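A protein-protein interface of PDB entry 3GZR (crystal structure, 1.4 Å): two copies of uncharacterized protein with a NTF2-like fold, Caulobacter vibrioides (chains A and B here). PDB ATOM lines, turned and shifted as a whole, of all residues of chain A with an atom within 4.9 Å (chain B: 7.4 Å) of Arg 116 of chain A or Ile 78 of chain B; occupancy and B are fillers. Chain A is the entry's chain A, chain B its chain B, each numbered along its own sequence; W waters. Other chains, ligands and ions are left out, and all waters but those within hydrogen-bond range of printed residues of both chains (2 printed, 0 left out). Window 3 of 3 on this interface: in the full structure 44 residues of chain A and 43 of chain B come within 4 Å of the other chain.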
ATOM      1  N   TRP A  32      21.117  -7.245  20.587  1.00  0.00           N
ATOM      2  CA  TRP A  32      21.288  -7.029  22.011  1.00  0.00           C
ATOM      3  C   TRP A  32      22.524  -7.827  22.470  1.00  0.00           C
ATOM      4  O   TRP A  32      22.866  -8.878  21.889  1.00  0.00           O
ATOM      5  CB  TRP A  32      20.067  -7.507  22.805  1.00  0.00           C
ATOM      6  CG  TRP A  32      18.861  -6.671  22.547  1.00  0.00           C
ATOM      7  CD1 TRP A  32      17.698  -7.095  21.962  1.00  0.00           C
ATOM      8  CD2 TRP A  32      18.704  -5.266  22.791  1.00  0.00           C
ATOM      9  NE1 TRP A  32      16.815  -6.035  21.855  1.00  0.00           N
ATOM     10  CE2 TRP A  32      17.410  -4.914  22.363  1.00  0.00           C
ATOM     11  CE3 TRP A  32      19.523  -4.280  23.357  1.00  0.00           C
ATOM     12  CZ2 TRP A  32      16.920  -3.602  22.450  1.00  0.00           C
ATOM     13  CZ3 TRP A  32      19.027  -2.968  23.457  1.00  0.00           C
ATOM     14  CH2 TRP A  32      17.745  -2.650  22.990  1.00  0.00           C
ATOM     15  N   ASP A  34      22.896  -9.853  24.884  1.00  0.00           N
ATOM     16  CA  ASP A  34      22.447 -11.194  25.290  1.00  0.00           C
ATOM     17  C   ASP A  34      21.844 -12.000  24.129  1.00  0.00           C
ATOM     18  O   ASP A  34      21.157 -12.991  24.371  1.00  0.00           O
ATOM     19  CB  ASP A  34      21.505 -11.110  26.525  1.00  0.00           C
ATOM     20  CG  ASP A  34      20.341 -10.149  26.372  1.00  0.00           C
ATOM     21  OD1 ASP A  34      20.565  -8.975  25.948  1.00  0.00           O
ATOM     22  OD2 ASP A  34      19.202 -10.536  26.754  1.00  0.00           O
ATOM     23  N   LEU A 112      14.322 -13.132  15.709  1.00  0.00           N
ATOM     24  CA  LEU A 112      13.491 -12.645  16.800  1.00  0.00           C
ATOM     25  C   LEU A 112      14.057 -11.304  17.271  1.00  0.00           C
ATOM     26  O   LEU A 112      15.290 -11.217  17.511  1.00  0.00           O
ATOM     27  CB  LEU A 112      13.465 -13.680  17.912  1.00  0.00           C
ATOM     28  CG  LEU A 112      12.607 -13.325  19.117  1.00  0.00           C
ATOM     29  CD1 LEU A 112      11.142 -13.157  18.735  1.00  0.00           C
ATOM     30  CD2 LEU A 112      12.802 -14.425  20.180  1.00  0.00           C
ATOM     31  N   VAL A 114      13.379  -7.982  20.045  1.00  0.00           N
ATOM     32  CA  VAL A 114      12.672  -7.506  21.225  1.00  0.00           C
ATOM     33  C   VAL A 114      12.980  -6.011  21.422  1.00  0.00           C
ATOM     34  O   VAL A 114      14.069  -5.512  21.057  1.00  0.00           O
ATOM     35  CB  VAL A 114      12.991  -8.307  22.501  1.00  0.00           C
ATOM     36  CG1 VAL A 114      12.539  -9.804  22.377  1.00  0.00           C
ATOM     37  CG2 VAL A 114      14.463  -8.260  22.858  1.00  0.00           C
ATOM     38  N   GLU A 115      11.990  -5.343  22.012  1.00  0.00           N
ATOM     39  CA  GLU A 115      12.034  -3.905  22.272  1.00  0.00           C
ATOM     40  C   GLU A 115      12.414  -3.641  23.721  1.00  0.00           C
ATOM     41  O   GLU A 115      11.794  -4.192  24.622  1.00  0.00           O
ATOM     42  CB  GLU A 115      10.675  -3.326  22.001  1.00  0.00           C
ATOM     43  CG  GLU A 115      10.663  -1.803  21.987  1.00  0.00           C
ATOM     44  CD  GLU A 115       9.293  -1.190  21.811  1.00  0.00           C
ATOM     45  OE1 GLU A 115       8.246  -1.903  21.860  1.00  0.00           O
ATOM     46  OE2 GLU A 115       9.259   0.077  21.694  1.00  0.00           O
ATOM     47  N   ARG A 116      13.421  -2.807  23.937  1.00  0.00           N
ATOM     48  CA  ARG A 116      13.865  -2.417  25.286  1.00  0.00           C
ATOM     49  C   ARG A 116      14.102  -0.914  25.289  1.00  0.00           C
ATOM     50  O   ARG A 116      14.799  -0.392  24.420  1.00  0.00           O
ATOM     51  CB  ARG A 116      15.129  -3.156  25.713  1.00  0.00           C
ATOM     52  CG  ARG A 116      14.984  -4.644  25.669  1.00  0.00           C
ATOM     53  CD  ARG A 116      16.266  -5.310  25.957  1.00  0.00           C
ATOM     54  NE  ARG A 116      16.118  -6.767  25.980  1.00  0.00           N
ATOM     55  CZ  ARG A 116      17.125  -7.646  26.088  1.00  0.00           C
ATOM     56  NH1 ARG A 116      18.384  -7.224  26.138  1.00  0.00           N
ATOM     57  NH2 ARG A 116      16.845  -8.949  26.146  1.00  0.00           N
ATOM     58  N   GLU A 117      13.461  -0.236  26.239  1.00  0.00           N
ATOM     59  CA  GLU A 117      13.583   1.225  26.361  1.00  0.00           C
ATOM     60  C   GLU A 117      13.254   1.908  25.006  1.00  0.00           C
ATOM     61  O   GLU A 117      13.922   2.862  24.592  1.00  0.00           O
ATOM     62  CB  GLU A 117      14.976   1.638  26.856  1.00  0.00           C
ATOM     63  CG  GLU A 117      15.497   0.906  28.107  1.00  0.00           C
ATOM     64  CD  GLU A 117      14.731   1.209  29.385  1.00  0.00           C
ATOM     65  OE1 GLU A 117      14.124   2.300  29.495  1.00  0.00           O
ATOM     66  OE2 GLU A 117      14.764   0.352  30.309  1.00  0.00           O
ATOM     67  N   GLY A 118      12.248   1.365  24.309  1.00  0.00           N
ATOM     68  CA  GLY A 118      11.783   1.933  23.037  1.00  0.00           C
ATOM     69  C   GLY A 118      12.574   1.618  21.775  1.00  0.00           C
ATOM     70  O   GLY A 118      12.216   2.146  20.696  1.00  0.00           O
ATOM     71  N   VAL A 119      13.612   0.787  21.891  1.00  0.00           N
ATOM     72  CA  VAL A 119      14.540   0.460  20.813  1.00  0.00           C
ATOM     73  C   VAL A 119      14.435  -1.041  20.522  1.00  0.00           C
ATOM     74  O   VAL A 119      14.314  -1.834  21.444  1.00  0.00           O
ATOM     75  CB  VAL A 119      16.014   0.763  21.268  1.00  0.00           C
ATOM     76  CG1 VAL A 119      17.017   0.276  20.284  1.00  0.00           C
ATOM     77  CG2 VAL A 119      16.212   2.280  21.563  1.00  0.00           C
ATOM     78  N   ILE A 123      17.469 -10.481  19.154  1.00  0.00           N
ATOM     79  CA  ILE A 123      17.868 -11.335  20.299  1.00  0.00           C
ATOM     80  C   ILE A 123      18.246 -12.750  19.862  1.00  0.00           C
ATOM     81  O   ILE A 123      18.972 -13.432  20.585  1.00  0.00           O
ATOM     82  CB  ILE A 123      16.784 -11.317  21.404  1.00  0.00           C
ATOM     83  CG1 ILE A 123      17.291 -11.806  22.772  1.00  0.00           C
ATOM     84  CG2 ILE A 123      15.555 -12.119  20.957  1.00  0.00           C
ATOM     85  CD1 ILE A 123      18.379 -10.927  23.386  1.00  0.00           C
ATOM     86  N   ARG B  76      16.718 -19.331  28.690  1.00  0.00           N
ATOM     87  CA  ARG B  76      16.864 -18.019  29.293  1.00  0.00           C
ATOM     88  C   ARG B  76      15.651 -17.139  29.028  1.00  0.00           C
ATOM     89  O   ARG B  76      14.938 -17.288  28.048  1.00  0.00           O
ATOM     90  CB  ARG B  76      18.148 -17.331  28.803  1.00  0.00           C
ATOM     91  CG  ARG B  76      18.093 -16.824  27.370  1.00  0.00           C
ATOM     92  CD  ARG B  76      19.443 -16.293  26.975  1.00  0.00           C
ATOM     93  NE  ARG B  76      19.415 -15.446  25.754  1.00  0.00           N
ATOM     94  CZ  ARG B  76      19.429 -15.911  24.499  1.00  0.00           C
ATOM     95  NH1 ARG B  76      19.439 -17.206  24.226  1.00  0.00           N
ATOM     96  NH2 ARG B  76      19.427 -15.056  23.490  1.00  0.00           N
ATOM     97  N   THR B  77      15.458 -16.174  29.907  1.00  0.00           N
ATOM     98  CA  THR B  77      14.480 -15.119  29.682  1.00  0.00           C
ATOM     99  C   THR B  77      15.040 -14.097  28.688  1.00  0.00           C
ATOM    100  O   THR B  77      16.232 -13.757  28.714  1.00  0.00           O
ATOM    101  CB  THR B  77      14.113 -14.484  31.025  1.00  0.00           C
ATOM    102  OG1 THR B  77      13.459 -15.484  31.814  1.00  0.00           O
ATOM    103  CG2 THR B  77      13.171 -13.281  30.848  1.00  0.00           C
ATOM    104  N   ILE B  78      14.203 -13.649  27.755  1.00  0.00           N
ATOM    105  CA  ILE B  78      14.544 -12.597  26.819  1.00  0.00           C
ATOM    106  C   ILE B  78      13.694 -11.309  26.910  1.00  0.00           C
ATOM    107  O   ILE B  78      14.081 -10.289  26.367  1.00  0.00           O
ATOM    108  CB  ILE B  78      14.559 -13.117  25.339  1.00  0.00           C
ATOM    109  CG1 ILE B  78      13.180 -13.645  24.942  1.00  0.00           C
ATOM    110  CG2 ILE B  78      15.678 -14.127  25.165  1.00  0.00           C
ATOM    111  CD1 ILE B  78      13.038 -13.903  23.437  1.00  0.00           C
ATOM    112  N   ALA B  79      12.531 -11.414  27.558  1.00  0.00           N
ATOM    113  CA  ALA B  79      11.620 -10.290  27.839  1.00  0.00           C
ATOM    114  C   ALA B  79      10.669 -10.780  28.907  1.00  0.00           C
ATOM    115  O   ALA B  79      10.544 -11.987  29.113  1.00  0.00           O
ATOM    116  CB  ALA B  79      10.834  -9.911  26.577  1.00  0.00           C
ATOM    117  N   PRO B  80       9.956  -9.891  29.619  1.00  0.00           N
ATOM    118  CA  PRO B  80       8.979 -10.401  30.556  1.00  0.00           C
ATOM    119  C   PRO B  80       7.935 -11.274  29.825  1.00  0.00           C
ATOM    120  O   PRO B  80       7.424 -10.871  28.758  1.00  0.00           O
ATOM    121  CB  PRO B  80       8.330  -9.136  31.124  1.00  0.00           C
ATOM    122  CG  PRO B  80       9.404  -8.109  30.952  1.00  0.00           C
ATOM    123  CD  PRO B  80      10.099  -8.426  29.706  1.00  0.00           C
ATOM    124  N   GLY B  81       7.721 -12.476  30.333  1.00  0.00           N
ATOM    125  CA  GLY B  81       6.815 -13.383  29.670  1.00  0.00           C
ATOM    126  C   GLY B  81       7.312 -14.048  28.397  1.00  0.00           C
ATOM    127  O   GLY B  81       6.503 -14.560  27.630  1.00  0.00           O
ATOM    128  N   SER B  82       8.624 -14.001  28.151  1.00  0.00           N
ATOM    129  CA  SER B  82       9.208 -14.640  26.966  1.00  0.00           C
ATOM    130  C   SER B  82      10.480 -15.385  27.333  1.00  0.00           C
ATOM    131  O   SER B  82      11.421 -14.789  27.910  1.00  0.00           O
ATOM    132  CB  SER B  82       9.481 -13.606  25.892  1.00  0.00           C
ATOM    133  OG  SER B  82       9.881 -14.224  24.679  1.00  0.00           O
ATOM    134  N   ALA B  83      10.543 -16.678  26.989  1.00  0.00           N
ATOM    135  CA  ALA B  83      11.676 -17.528  27.307  1.00  0.00           C
ATOM    136  C   ALA B  83      12.121 -18.266  26.049  1.00  0.00           C
ATOM    137  O   ALA B  83      11.287 -18.783  25.280  1.00  0.00           O
ATOM    138  CB  ALA B  83      11.288 -18.533  28.410  1.00  0.00           C
ATOM    139  N   LEU B  84      13.419 -18.307  25.851  1.00  0.00           N
ATOM    140  CA  LEU B  84      14.053 -18.876  24.682  1.00  0.00           C
ATOM    141  C   LEU B  84      14.961 -20.006  25.132  1.00  0.00           C
ATOM    142  O   LEU B  84      15.791 -19.835  26.018  1.00  0.00           O
ATOM    143  CB  LEU B  84      14.824 -17.773  23.968  1.00  0.00           C
ATOM    144  CG  LEU B  84      15.649 -18.164  22.762  1.00  0.00           C
ATOM    145  CD1 LEU B  84      14.770 -18.701  21.665  1.00  0.00           C
ATOM    146  CD2 LEU B  84      16.438 -16.955  22.251  1.00  0.00           C
ATOM    147  N   ALA B  85      14.855 -21.145  24.463  1.00  0.00           N
ATOM    148  CA  ALA B  85      15.749 -22.266  24.727  1.00  0.00           C
ATOM    149  C   ALA B  85      16.403 -22.716  23.439  1.00  0.00           C
ATOM    150  O   ALA B  85      15.759 -22.759  22.372  1.00  0.00           O
ATOM    151  CB  ALA B  85      14.988 -23.457  25.341  1.00  0.00           C
ATOM    152  N   LEU B 112      10.755 -21.288  21.521  1.00  0.00           N
ATOM    153  CA  LEU B 112      10.381 -19.976  22.081  1.00  0.00           C
ATOM    154  C   LEU B 112       9.015 -20.121  22.700  1.00  0.00           C
ATOM    155  O   LEU B 112       8.074 -20.558  22.024  1.00  0.00           O
ATOM    156  CB  LEU B 112      10.352 -18.911  20.983  1.00  0.00           C
ATOM    157  CG  LEU B 112       9.994 -17.497  21.423  1.00  0.00           C
ATOM    158  CD1 LEU B 112      10.980 -16.935  22.449  1.00  0.00           C
ATOM    159  CD2 LEU B 112       9.881 -16.591  20.176  1.00  0.00           C
ATOM    160  N   ALA B 113       8.925 -19.774  23.998  1.00  0.00           N
ATOM    161  CA  ALA B 113       7.661 -19.820  24.742  1.00  0.00           C
ATOM    162  C   ALA B 113       7.287 -18.427  25.199  1.00  0.00           C
ATOM    163  O   ALA B 113       8.146 -17.638  25.567  1.00  0.00           O
ATOM    164  CB  ALA B 113       7.780 -20.762  25.921  1.00  0.00           C
ATOM    165  N   VAL B 114       5.993 -18.125  25.167  1.00  0.00           N
ATOM    166  CA  VAL B 114       5.477 -16.861  25.652  1.00  0.00           C
ATOM    167  C   VAL B 114       4.327 -17.140  26.631  1.00  0.00           C
ATOM    168  O   VAL B 114       3.603 -18.148  26.511  1.00  0.00           O
ATOM    169  CB  VAL B 114       5.064 -15.868  24.561  1.00  0.00           C
ATOM    170  CG1 VAL B 114       6.313 -15.471  23.698  1.00  0.00           C
ATOM    171  CG2 VAL B 114       3.893 -16.349  23.715  1.00  0.00           C
HETATM  172  O   HOH W   1      13.344  -7.692  26.316  1.00  0.00           O
HETATM  173  O   HOH W   2      18.668 -13.143  27.321  1.00  0.00           O
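The side-chain carboxylate (OD1) of Asp 34 of chain A lies within salt-bridge range of the guanidinium group (NH1) of Arg 116 of chain A.
The backbone NH (N) of Ile 123 of chain A sits at hydrogen-bond distance from the backbone carbonyl oxygen (O) of Leu 112 of chain A, at 2.8 Å.
N of Leu 84 of chain B lies within hydrogen-bond range of O of Arg 76 of chain B.
Leu 112 of chain A touches its own counterpart, Leu 112 of chain B.
2 positions are printed for both chains.
Of the 6 pairs that touch across the chains among the printed residues, 1 has its exchanged pair printed and touching as well.
Water W1 lies within hydrogen-bond range of the backbone carbonyl oxygen (O) of Ile 78 of chain B (2.7 Å) and the guanidinium group (NE) of Arg 116 of chain A (2.9 Å).
Water W2 lies within hydrogen-bond range of the side-chain carboxylate of Asp 34 of chain A (2.7 Å), the backbone carbonyl oxygen of Thr 77 of chain B (2.9 Å) and the guanidinium group of Arg 76 of chain B (2.9 Å).
Of the printed residues of chain B, Asp 34 of chain A touches Arg 76.
Printed residues of chain B within 4 Å of Leu 112 of chain A: Ile 78 (3.3 Å) and Leu 112 (3.6 Å).
Glu 115 of chain A touches none of the printed residues of chain B.
Arg 116 of chain A touches just one residue of chain B: Ile 78.
Gly 118 of chain A touches none of the printed residues of chain B.
Printed residues of chain A within 4 Å of Arg 76 of chain B: Asp 34 (2.8 Å) and Ile 123 (3.4 Å).
Printed residues of chain A within 4 Å of Ile 78 of chain B: Leu 112, Arg 116 and Ile 123.
Of the printed residues of chain A, Leu 112 of chain B touches Leu 112 (3.6 Å).
The nearest printed residue of chain A that does not touch Ile 78 of chain B is Val 114 of chain A (4.1 Å).
The nearest printed residue of chain A that does not touch Arg 76 of chain B is Arg 116 of chain A (7.0 Å).
NH2 of Arg 76 of chain B lies within hydrogen-bond range of O of Asp 34 of chain A (2.8 Å).
O of Ile 78 of chain B is in hydrogen-bond range of NH2 of Arg 116 of chain A (3.1 Å).
NH2 of Arg 76 of chain B sits at hydrogen-bond distance from O of Ile 123 of chain A, at 3.4 Å.
Among the printed residues, merely in contact across the chains: Leu 112 of chain A with Ile 78 of chain B, Leu 112 of chain A with Leu 112 of chain B and Ile 123 of chain A with Ile 78 of chain B.
Hydrophobic or aromatic side chains of chain B that line the printed part of chain A: Ile 78 and Leu 112.
Printed residues of chain A that touch a printed residue of chain B: Asp 34, Leu 112, Arg 116 and Ile 123.
Along chain A the printed residues that touch a printed residue of chain B span positions 34 to 123.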
